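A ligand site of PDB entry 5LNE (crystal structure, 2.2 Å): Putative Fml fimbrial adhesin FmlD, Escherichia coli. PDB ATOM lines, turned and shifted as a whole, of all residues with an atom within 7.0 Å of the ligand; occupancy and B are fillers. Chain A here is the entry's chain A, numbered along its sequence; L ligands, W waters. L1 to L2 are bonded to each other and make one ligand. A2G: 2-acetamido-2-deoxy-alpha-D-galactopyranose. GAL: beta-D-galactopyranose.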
ATOM      1  N   PHE A   1      11.529   3.540 -15.906  1.00  0.00           N
ATOM      2  CA  PHE A   1      10.396   4.335 -16.485  1.00  0.00           C
ATOM      3  C   PHE A   1       9.308   3.341 -16.940  1.00  0.00           C
ATOM      4  O   PHE A   1       9.657   2.318 -17.578  1.00  0.00           O
ATOM      5  CB  PHE A   1      10.910   5.143 -17.685  1.00  0.00           C
ATOM      6  CG  PHE A   1       9.838   5.902 -18.416  1.00  0.00           C
ATOM      7  CD1 PHE A   1       9.259   7.054 -17.848  1.00  0.00           C
ATOM      8  CD2 PHE A   1       9.456   5.506 -19.676  1.00  0.00           C
ATOM      9  CE1 PHE A   1       8.298   7.753 -18.528  1.00  0.00           C
ATOM     10  CE2 PHE A   1       8.511   6.211 -20.370  1.00  0.00           C
ATOM     11  CZ  PHE A   1       7.910   7.327 -19.786  1.00  0.00           C
ATOM     12  N   SER A   2       8.035   3.624 -16.650  1.00  0.00           N
ATOM     13  CA  SER A   2       6.953   2.751 -17.047  1.00  0.00           C
ATOM     14  C   SER A   2       5.833   3.572 -17.687  1.00  0.00           C
ATOM     15  O   SER A   2       5.698   4.718 -17.370  1.00  0.00           O
ATOM     16  CB  SER A   2       6.395   2.049 -15.827  1.00  0.00           C
ATOM     17  OG  SER A   2       7.425   1.358 -15.183  1.00  0.00           O
ATOM     18  N   SER A  10       2.053  -2.687 -16.840  1.00  0.00           N
ATOM     19  CA  SER A  10       3.046  -1.672 -17.054  1.00  0.00           C
ATOM     20  C   SER A  10       3.922  -2.096 -18.277  1.00  0.00           C
ATOM     21  O   SER A  10       4.025  -3.256 -18.617  1.00  0.00           O
ATOM     22  CB  SER A  10       3.837  -1.480 -15.771  1.00  0.00           C
ATOM     23  OG  SER A  10       4.726  -2.549 -15.687  1.00  0.00           O
ATOM     24  N   GLY A  12       7.568  -1.277 -20.523  1.00  0.00           N
ATOM     25  CA  GLY A  12       8.912  -0.751 -20.376  1.00  0.00           C
ATOM     26  C   GLY A  12       9.535  -0.349 -21.716  1.00  0.00           C
ATOM     27  O   GLY A  12      10.522   0.354 -21.713  1.00  0.00           O
ATOM     28  N   TRP A  43       5.208   7.056 -15.738  1.00  0.00           N
ATOM     29  CA  TRP A  43       5.722   7.526 -14.490  1.00  0.00           C
ATOM     30  C   TRP A  43       7.191   7.102 -14.264  1.00  0.00           C
ATOM     31  O   TRP A  43       7.709   6.202 -14.908  1.00  0.00           O
ATOM     32  CB  TRP A  43       4.798   7.014 -13.333  1.00  0.00           C
ATOM     33  CG  TRP A  43       4.683   5.477 -13.209  1.00  0.00           C
ATOM     34  CD1 TRP A  43       5.479   4.689 -12.475  1.00  0.00           C
ATOM     35  CD2 TRP A  43       3.758   4.596 -13.921  1.00  0.00           C
ATOM     36  NE1 TRP A  43       5.130   3.370 -12.679  1.00  0.00           N
ATOM     37  CE2 TRP A  43       4.068   3.286 -13.525  1.00  0.00           C
ATOM     38  CE3 TRP A  43       2.745   4.809 -14.881  1.00  0.00           C
ATOM     39  CZ2 TRP A  43       3.364   2.166 -14.020  1.00  0.00           C
ATOM     40  CZ3 TRP A  43       2.060   3.745 -15.360  1.00  0.00           C
ATOM     41  CH2 TRP A  43       2.353   2.431 -14.964  1.00  0.00           C
ATOM     42  N   ASN A  44       7.856   7.802 -13.347  1.00  0.00           N
ATOM     43  CA  ASN A  44       9.186   7.482 -12.890  1.00  0.00           C
ATOM     44  C   ASN A  44       9.062   6.336 -11.942  1.00  0.00           C
ATOM     45  O   ASN A  44       8.191   6.348 -11.073  1.00  0.00           O
ATOM     46  CB  ASN A  44       9.808   8.688 -12.219  1.00  0.00           C
ATOM     47  CG  ASN A  44      11.305   8.545 -11.951  1.00  0.00           C
ATOM     48  OD1 ASN A  44      11.731   7.807 -11.032  1.00  0.00           O
ATOM     49  ND2 ASN A  44      12.115   9.152 -12.829  1.00  0.00           N
ATOM     50  N   ASP A  45       9.888   5.326 -12.103  1.00  0.00           N
ATOM     51  CA  ASP A  45       9.814   4.137 -11.236  1.00  0.00           C
ATOM     52  C   ASP A  45      10.411   4.355  -9.842  1.00  0.00           C
ATOM     53  O   ASP A  45      10.159   3.543  -9.002  1.00  0.00           O
ATOM     54  CB  ASP A  45      10.413   2.879 -11.895  1.00  0.00           C
ATOM     55  CG  ASP A  45       9.575   2.380 -13.074  1.00  0.00           C
ATOM     56  OD1 ASP A  45       8.348   2.399 -13.005  1.00  0.00           O
ATOM     57  OD2 ASP A  45      10.109   2.019 -14.131  1.00  0.00           O
ATOM     58  N   TYR A  46      11.205   5.383  -9.581  1.00  0.00           N
ATOM     59  CA  TYR A  46      11.693   5.621  -8.202  1.00  0.00           C
ATOM     60  C   TYR A  46      11.024   6.809  -7.467  1.00  0.00           C
ATOM     61  O   TYR A  46      10.877   6.778  -6.261  1.00  0.00           O
ATOM     62  CB  TYR A  46      13.172   5.907  -8.195  1.00  0.00           C
ATOM     63  CG  TYR A  46      14.075   4.906  -8.896  1.00  0.00           C
ATOM     64  CD1 TYR A  46      13.862   3.543  -8.810  1.00  0.00           C
ATOM     65  CD2 TYR A  46      15.186   5.353  -9.575  1.00  0.00           C
ATOM     66  CE1 TYR A  46      14.707   2.659  -9.453  1.00  0.00           C
ATOM     67  CE2 TYR A  46      16.043   4.496 -10.213  1.00  0.00           C
ATOM     68  CZ  TYR A  46      15.817   3.144 -10.154  1.00  0.00           C
ATOM     69  OH  TYR A  46      16.694   2.275 -10.773  1.00  0.00           O
ATOM     70  N   GLY A  47      10.677   7.893  -8.211  1.00  0.00           N
ATOM     71  CA  GLY A  47      10.165   9.092  -7.572  1.00  0.00           C
ATOM     72  C   GLY A  47      11.273  10.006  -7.032  1.00  0.00           C
ATOM     73  O   GLY A  47      12.490   9.680  -7.097  1.00  0.00           O
ATOM     74  N   ASP A  51      16.347   9.826 -10.376  1.00  0.00           N
ATOM     75  CA  ASP A  51      16.839   9.417 -11.693  1.00  0.00           C
ATOM     76  C   ASP A  51      15.800   9.861 -12.696  1.00  0.00           C
ATOM     77  O   ASP A  51      14.956   9.092 -13.039  1.00  0.00           O
ATOM     78  CB  ASP A  51      17.064   7.894 -11.792  1.00  0.00           C
ATOM     79  CG  ASP A  51      17.834   7.503 -13.056  1.00  0.00           C
ATOM     80  OD1 ASP A  51      18.190   8.446 -13.760  1.00  0.00           O
ATOM     81  OD2 ASP A  51      18.086   6.297 -13.329  1.00  0.00           O
ATOM     82  N   THR A  52      15.870  11.116 -13.150  1.00  0.00           N
ATOM     83  CA  THR A  52      14.750  11.727 -13.862  1.00  0.00           C
ATOM     84  C   THR A  52      14.695  11.169 -15.319  1.00  0.00           C
ATOM     85  O   THR A  52      15.710  11.016 -15.937  1.00  0.00           O
ATOM     86  CB  THR A  52      14.851  13.242 -13.810  1.00  0.00           C
ATOM     87  OG1 THR A  52      14.826  13.731 -12.457  1.00  0.00           O
ATOM     88  CG2 THR A  52      13.744  13.939 -14.609  1.00  0.00           C
ATOM     89  N   ASP A  53      13.493  10.890 -15.807  1.00  0.00           N
ATOM     90  CA  ASP A  53      13.245  10.411 -17.136  1.00  0.00           C
ATOM     91  C   ASP A  53      12.941  11.551 -18.066  1.00  0.00           C
ATOM     92  O   ASP A  53      12.240  12.462 -17.717  1.00  0.00           O
ATOM     93  CB  ASP A  53      12.085   9.417 -17.114  1.00  0.00           C
ATOM     94  CG  ASP A  53      12.410   8.144 -16.309  1.00  0.00           C
ATOM     95  OD1 ASP A  53      13.453   7.503 -16.685  1.00  0.00           O
ATOM     96  OD2 ASP A  53      11.633   7.756 -15.371  1.00  0.00           O
ATOM     97  N   ILE A  94      10.066  13.542 -16.447  1.00  0.00           N
ATOM     98  CA  ILE A  94       9.204  12.808 -15.532  1.00  0.00           C
ATOM     99  C   ILE A  94      10.052  12.282 -14.379  1.00  0.00           C
ATOM    100  O   ILE A  94      10.905  11.376 -14.566  1.00  0.00           O
ATOM    101  CB  ILE A  94       8.439  11.704 -16.289  1.00  0.00           C
ATOM    102  CG1 ILE A  94       7.368  12.341 -17.228  1.00  0.00           C
ATOM    103  CG2 ILE A  94       7.720  10.745 -15.354  1.00  0.00           C
ATOM    104  CD1 ILE A  94       6.929  11.446 -18.338  1.00  0.00           C
ATOM    105  N   LYS A  97       6.719   9.257  -9.144  1.00  0.00           N
ATOM    106  CA  LYS A  97       6.097   7.973  -9.211  1.00  0.00           C
ATOM    107  C   LYS A  97       4.574   8.123  -9.176  1.00  0.00           C
ATOM    108  O   LYS A  97       3.919   7.597  -8.280  1.00  0.00           O
ATOM    109  CB  LYS A  97       6.553   7.198  -8.012  1.00  0.00           C
ATOM    110  CG  LYS A  97       6.480   5.721  -8.102  1.00  0.00           C
ATOM    111  CD  LYS A  97       7.178   5.184  -6.860  1.00  0.00           C
ATOM    112  CE  LYS A  97       6.753   3.814  -6.410  1.00  0.00           C
ATOM    113  NZ  LYS A  97       7.270   2.900  -7.444  1.00  0.00           N
ATOM    114  N   LYS A 132      12.760   7.428 -24.547  1.00  0.00           N
ATOM    115  CA  LYS A 132      13.048   7.697 -23.206  1.00  0.00           C
ATOM    116  C   LYS A 132      14.511   7.485 -22.964  1.00  0.00           C
ATOM    117  O   LYS A 132      15.062   6.506 -23.421  1.00  0.00           O
ATOM    118  CB  LYS A 132      12.264   6.685 -22.300  1.00  0.00           C
ATOM    119  CG  LYS A 132      12.760   6.636 -20.829  1.00  0.00           C
ATOM    120  CD  LYS A 132      13.601   5.346 -20.488  1.00  0.00           C
ATOM    121  CE  LYS A 132      14.368   5.574 -19.220  1.00  0.00           C
ATOM    122  NZ  LYS A 132      15.104   4.402 -18.689  1.00  0.00           N
ATOM    123  N   ILE A 133      15.139   8.385 -22.211  1.00  0.00           N
ATOM    124  CA  ILE A 133      16.416   8.152 -21.593  1.00  0.00           C
ATOM    125  C   ILE A 133      16.362   8.881 -20.197  1.00  0.00           C
ATOM    126  O   ILE A 133      15.699   9.904 -20.023  1.00  0.00           O
ATOM    127  CB  ILE A 133      17.520   8.701 -22.469  1.00  0.00           C
ATOM    128  CG1 ILE A 133      18.883   8.359 -21.902  1.00  0.00           C
ATOM    129  CG2 ILE A 133      17.404  10.215 -22.684  1.00  0.00           C
ATOM    130  CD1 ILE A 133      20.024   8.506 -22.873  1.00  0.00           C
ATOM    131  N   ALA A 134      17.051   8.337 -19.222  1.00  0.00           N
ATOM    132  CA  ALA A 134      17.045   8.908 -17.884  1.00  0.00           C
ATOM    133  C   ALA A 134      18.363   9.656 -17.659  1.00  0.00           C
ATOM    134  O   ALA A 134      18.986  10.082 -18.601  1.00  0.00           O
ATOM    135  CB  ALA A 134      16.839   7.788 -16.863  1.00  0.00           C
ATOM    136  N   THR A 135      18.793   9.775 -16.408  1.00  0.00           N
ATOM    137  CA  THR A 135      19.835  10.697 -16.001  1.00  0.00           C
ATOM    138  C   THR A 135      21.132   9.943 -15.520  1.00  0.00           C
ATOM    139  O   THR A 135      22.230  10.356 -15.888  1.00  0.00           O
ATOM    140  CB  THR A 135      19.203  11.595 -14.887  1.00  0.00           C
ATOM    141  OG1 THR A 135      18.078  12.378 -15.418  1.00  0.00           O
ATOM    142  CG2 THR A 135      20.226  12.491 -14.269  1.00  0.00           C
ATOM    143  N   LEU A 136      20.985   8.859 -14.746  1.00  0.00           N
ATOM    144  CA  LEU A 136      22.117   8.129 -14.156  1.00  0.00           C
ATOM    145  C   LEU A 136      22.645   7.034 -15.064  1.00  0.00           C
ATOM    146  O   LEU A 136      21.917   6.501 -15.871  1.00  0.00           O
ATOM    147  CB  LEU A 136      21.716   7.520 -12.787  1.00  0.00           C
ATOM    148  CG  LEU A 136      21.097   8.471 -11.700  1.00  0.00           C
ATOM    149  CD1 LEU A 136      20.670   7.788 -10.416  1.00  0.00           C
ATOM    150  CD2 LEU A 136      22.051   9.610 -11.345  1.00  0.00           C
ATOM    151  N   SER A 138      24.138   5.020 -18.012  1.00  0.00           N
ATOM    152  CA  SER A 138      23.902   5.209 -19.445  1.00  0.00           C
ATOM    153  C   SER A 138      22.531   5.830 -19.724  1.00  0.00           C
ATOM    154  O   SER A 138      22.190   6.040 -20.855  1.00  0.00           O
ATOM    155  CB  SER A 138      23.890   3.832 -20.107  1.00  0.00           C
ATOM    156  OG  SER A 138      22.652   3.112 -19.775  1.00  0.00           O
ATOM    157  N   GLY A 139      21.690   5.984 -18.716  1.00  0.00           N
ATOM    158  CA  GLY A 139      20.316   6.437 -18.911  1.00  0.00           C
ATOM    159  C   GLY A 139      19.318   5.374 -19.330  1.00  0.00           C
ATOM    160  O   GLY A 139      18.109   5.700 -19.416  1.00  0.00           O
ATOM    161  N   ASN A 140      19.773   4.125 -19.574  1.00  0.00           N
ATOM    162  CA  ASN A 140      18.945   3.007 -20.065  1.00  0.00           C
ATOM    163  C   ASN A 140      17.842   3.416 -21.088  1.00  0.00           C
ATOM    164  O   ASN A 140      16.633   3.305 -20.820  1.00  0.00           O
ATOM    165  CB  ASN A 140      18.383   2.171 -18.898  1.00  0.00           C
ATOM    166  CG  ASN A 140      19.518   1.602 -18.012  1.00  0.00           C
ATOM    167  OD1 ASN A 140      19.449   1.622 -16.792  1.00  0.00           O
ATOM    168  ND2 ASN A 140      20.579   1.183 -18.629  1.00  0.00           N
ATOM    169  N   PRO A 141      18.278   3.898 -22.258  1.00  0.00           N
ATOM    170  CA  PRO A 141      17.320   4.315 -23.254  1.00  0.00           C
ATOM    171  C   PRO A 141      16.348   3.242 -23.690  1.00  0.00           C
ATOM    172  O   PRO A 141      16.707   2.089 -23.771  1.00  0.00           O
ATOM    173  CB  PRO A 141      18.203   4.796 -24.452  1.00  0.00           C
ATOM    174  CG  PRO A 141      19.577   4.223 -24.207  1.00  0.00           C
ATOM    175  CD  PRO A 141      19.675   3.831 -22.778  1.00  0.00           C
ATOM    176  N   ARG A 142      15.082   3.618 -23.924  1.00  0.00           N
ATOM    177  CA  ARG A 142      14.047   2.689 -24.375  1.00  0.00           C
ATOM    178  C   ARG A 142      13.254   3.293 -25.487  1.00  0.00           C
ATOM    179  O   ARG A 142      13.077   4.479 -25.500  1.00  0.00           O
ATOM    180  CB  ARG A 142      13.128   2.393 -23.194  1.00  0.00           C
ATOM    181  CG  ARG A 142      13.762   1.699 -22.036  1.00  0.00           C
ATOM    182  CD  ARG A 142      14.220   0.318 -22.498  1.00  0.00           C
ATOM    183  NE  ARG A 142      14.456  -0.626 -21.416  1.00  0.00           N
ATOM    184  CZ  ARG A 142      15.636  -0.811 -20.822  1.00  0.00           C
ATOM    185  NH1 ARG A 142      16.729  -0.127 -21.200  1.00  0.00           N
ATOM    186  NH2 ARG A 142      15.715  -1.704 -19.813  1.00  0.00           N
HETATM  187  O5  A2G L   1      12.656  -1.969 -11.707  1.00  0.00           O
HETATM  188  C1  A2G L   1      14.024  -1.628 -11.449  1.00  0.00           C
HETATM  189  O1  A2G L   1      14.018  -0.778 -10.313  1.00  0.00           O
HETATM  190  C2  A2G L   1      14.639  -0.828 -12.618  1.00  0.00           C
HETATM  191  N2  A2G L   1      15.983  -0.393 -12.321  1.00  0.00           N
HETATM  192  C3  A2G L   1      13.822   0.456 -12.925  1.00  0.00           C
HETATM  193  O3  A2G L   1      14.289   1.173 -14.118  1.00  0.00           O
HETATM  194  C4  A2G L   1      12.370   0.059 -13.082  1.00  0.00           C
HETATM  195  O4  A2G L   1      12.276  -0.637 -14.332  1.00  0.00           O
HETATM  196  C5  A2G L   1      11.837  -0.799 -11.926  1.00  0.00           C
HETATM  197  C6  A2G L   1      10.377  -1.182 -12.146  1.00  0.00           C
HETATM  198  O6  A2G L   1       9.906  -1.727 -10.900  1.00  0.00           O
HETATM  199  C7  A2G L   1      17.058  -0.767 -12.988  1.00  0.00           C
HETATM  200  O7  A2G L   1      16.942  -1.511 -13.958  1.00  0.00           O
HETATM  201  C8  A2G L   1      18.363  -0.171 -12.481  1.00  0.00           C
HETATM  202  C1  GAL L   2      14.779   2.409 -14.070  1.00  0.00           C
HETATM  203  C2  GAL L   2      15.643   2.748 -15.293  1.00  0.00           C
HETATM  204  C3  GAL L   2      16.189   4.145 -15.167  1.00  0.00           C
HETATM  205  C4  GAL L   2      15.122   5.184 -14.842  1.00  0.00           C
HETATM  206  C5  GAL L   2      14.450   4.794 -13.505  1.00  0.00           C
HETATM  207  C6  GAL L   2      13.315   5.752 -13.113  1.00  0.00           C
HETATM  208  O2  GAL L   2      16.717   1.785 -15.288  1.00  0.00           O
HETATM  209  O3  GAL L   2      16.856   4.438 -16.370  1.00  0.00           O
HETATM  210  O4  GAL L   2      14.154   5.260 -15.906  1.00  0.00           O
HETATM  211  O5  GAL L   2      13.905   3.478 -13.594  1.00  0.00           O
HETATM  212  O6  GAL L   2      12.177   5.577 -13.937  1.00  0.00           O
HETATM  213  O   HOH W   1      13.635  -0.235 -16.981  1.00  0.00           O
HETATM  214  O   HOH W   2      19.223   5.489 -15.448  1.00  0.00           O
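Water W2 lies within hydrogen-bond range of the side-chain carboxylate (OD2) of Asp 51 (2.5 Å), an oxygen (O3) of GAL L2 (2.7 Å) and the backbone carbonyl oxygen (O) of Leu 136 (2.9 Å).
The backbone NH of Ile 94 sits at hydrogen-bond distance from the backbone carbonyl oxygen of Asp 53, at 2.7 Å.
OD2 of Asp 45 is in hydrogen-bond range of N of Phe 1, at 2.7 Å.
The backbone carbonyl oxygen (O) of Asn 140 is in hydrogen-bond range of the guanidinium group (NH1) of Arg 142, 3.5 Å away.
The side-chain amide nitrogen of Asn 140 sits at hydrogen-bond distance from the side-chain hydroxyl of Ser 138 (3.1 Å).
The backbone NH (N) of Tyr 46 is in hydrogen-bond range of the side-chain amide oxygen (OD1) of Asn 44, 2.9 Å away.
The side-chain amide nitrogen of Asn 44 is in hydrogen-bond range of the backbone carbonyl oxygen of Ile 94 (3.1 Å).
N of Ala 134 lies within hydrogen-bond range of O of Gly 139, 2.8 Å away.
OD1 of Asp 51 sits at hydrogen-bond distance from N of Leu 136, at 3.0 Å.
Merely in contact with the ligand: Asn 44 (3.3 Å), Ala 134 (3.4 Å), Asp 51 (3.4 Å) and Gly 139 (3.5 Å).
Hydrophobic or aromatic side chains that line the ligand: Phe 1, Tyr 46 and Ala 134.
Of the 24 residues printed, 10 come within 4 Å of the ligand.
The nearest printed residue that does not touch the ligand is Trp 43 (4.6 Å).
An oxygen (O4) of GAL L2 lies within hydrogen-bond range of the side-chain carboxylate (OD1) of Asp 53.
N of Phe 1 lies within hydrogen-bond range of O6 of GAL L2 (2.9 Å).
The side-chain amino group (NZ) of Lys 132 is in hydrogen-bond range of an oxygen (O3) of GAL L2 (2.9 Å).
O6 of GAL L2 lies within hydrogen-bond range of N of Asp 45, 2.9 Å away.
OD2 of Asp 45 lies close to O4 of A2G L1 (3.4 Å).
An oxygen (O2) of GAL L2 sits at hydrogen-bond distance from the side-chain amide oxygen of Asn 140, at 3.1 Å.
The side-chain hydroxyl of Tyr 46 lies within hydrogen-bond range of a nitrogen (N2) of A2G L1 (3.2 Å).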
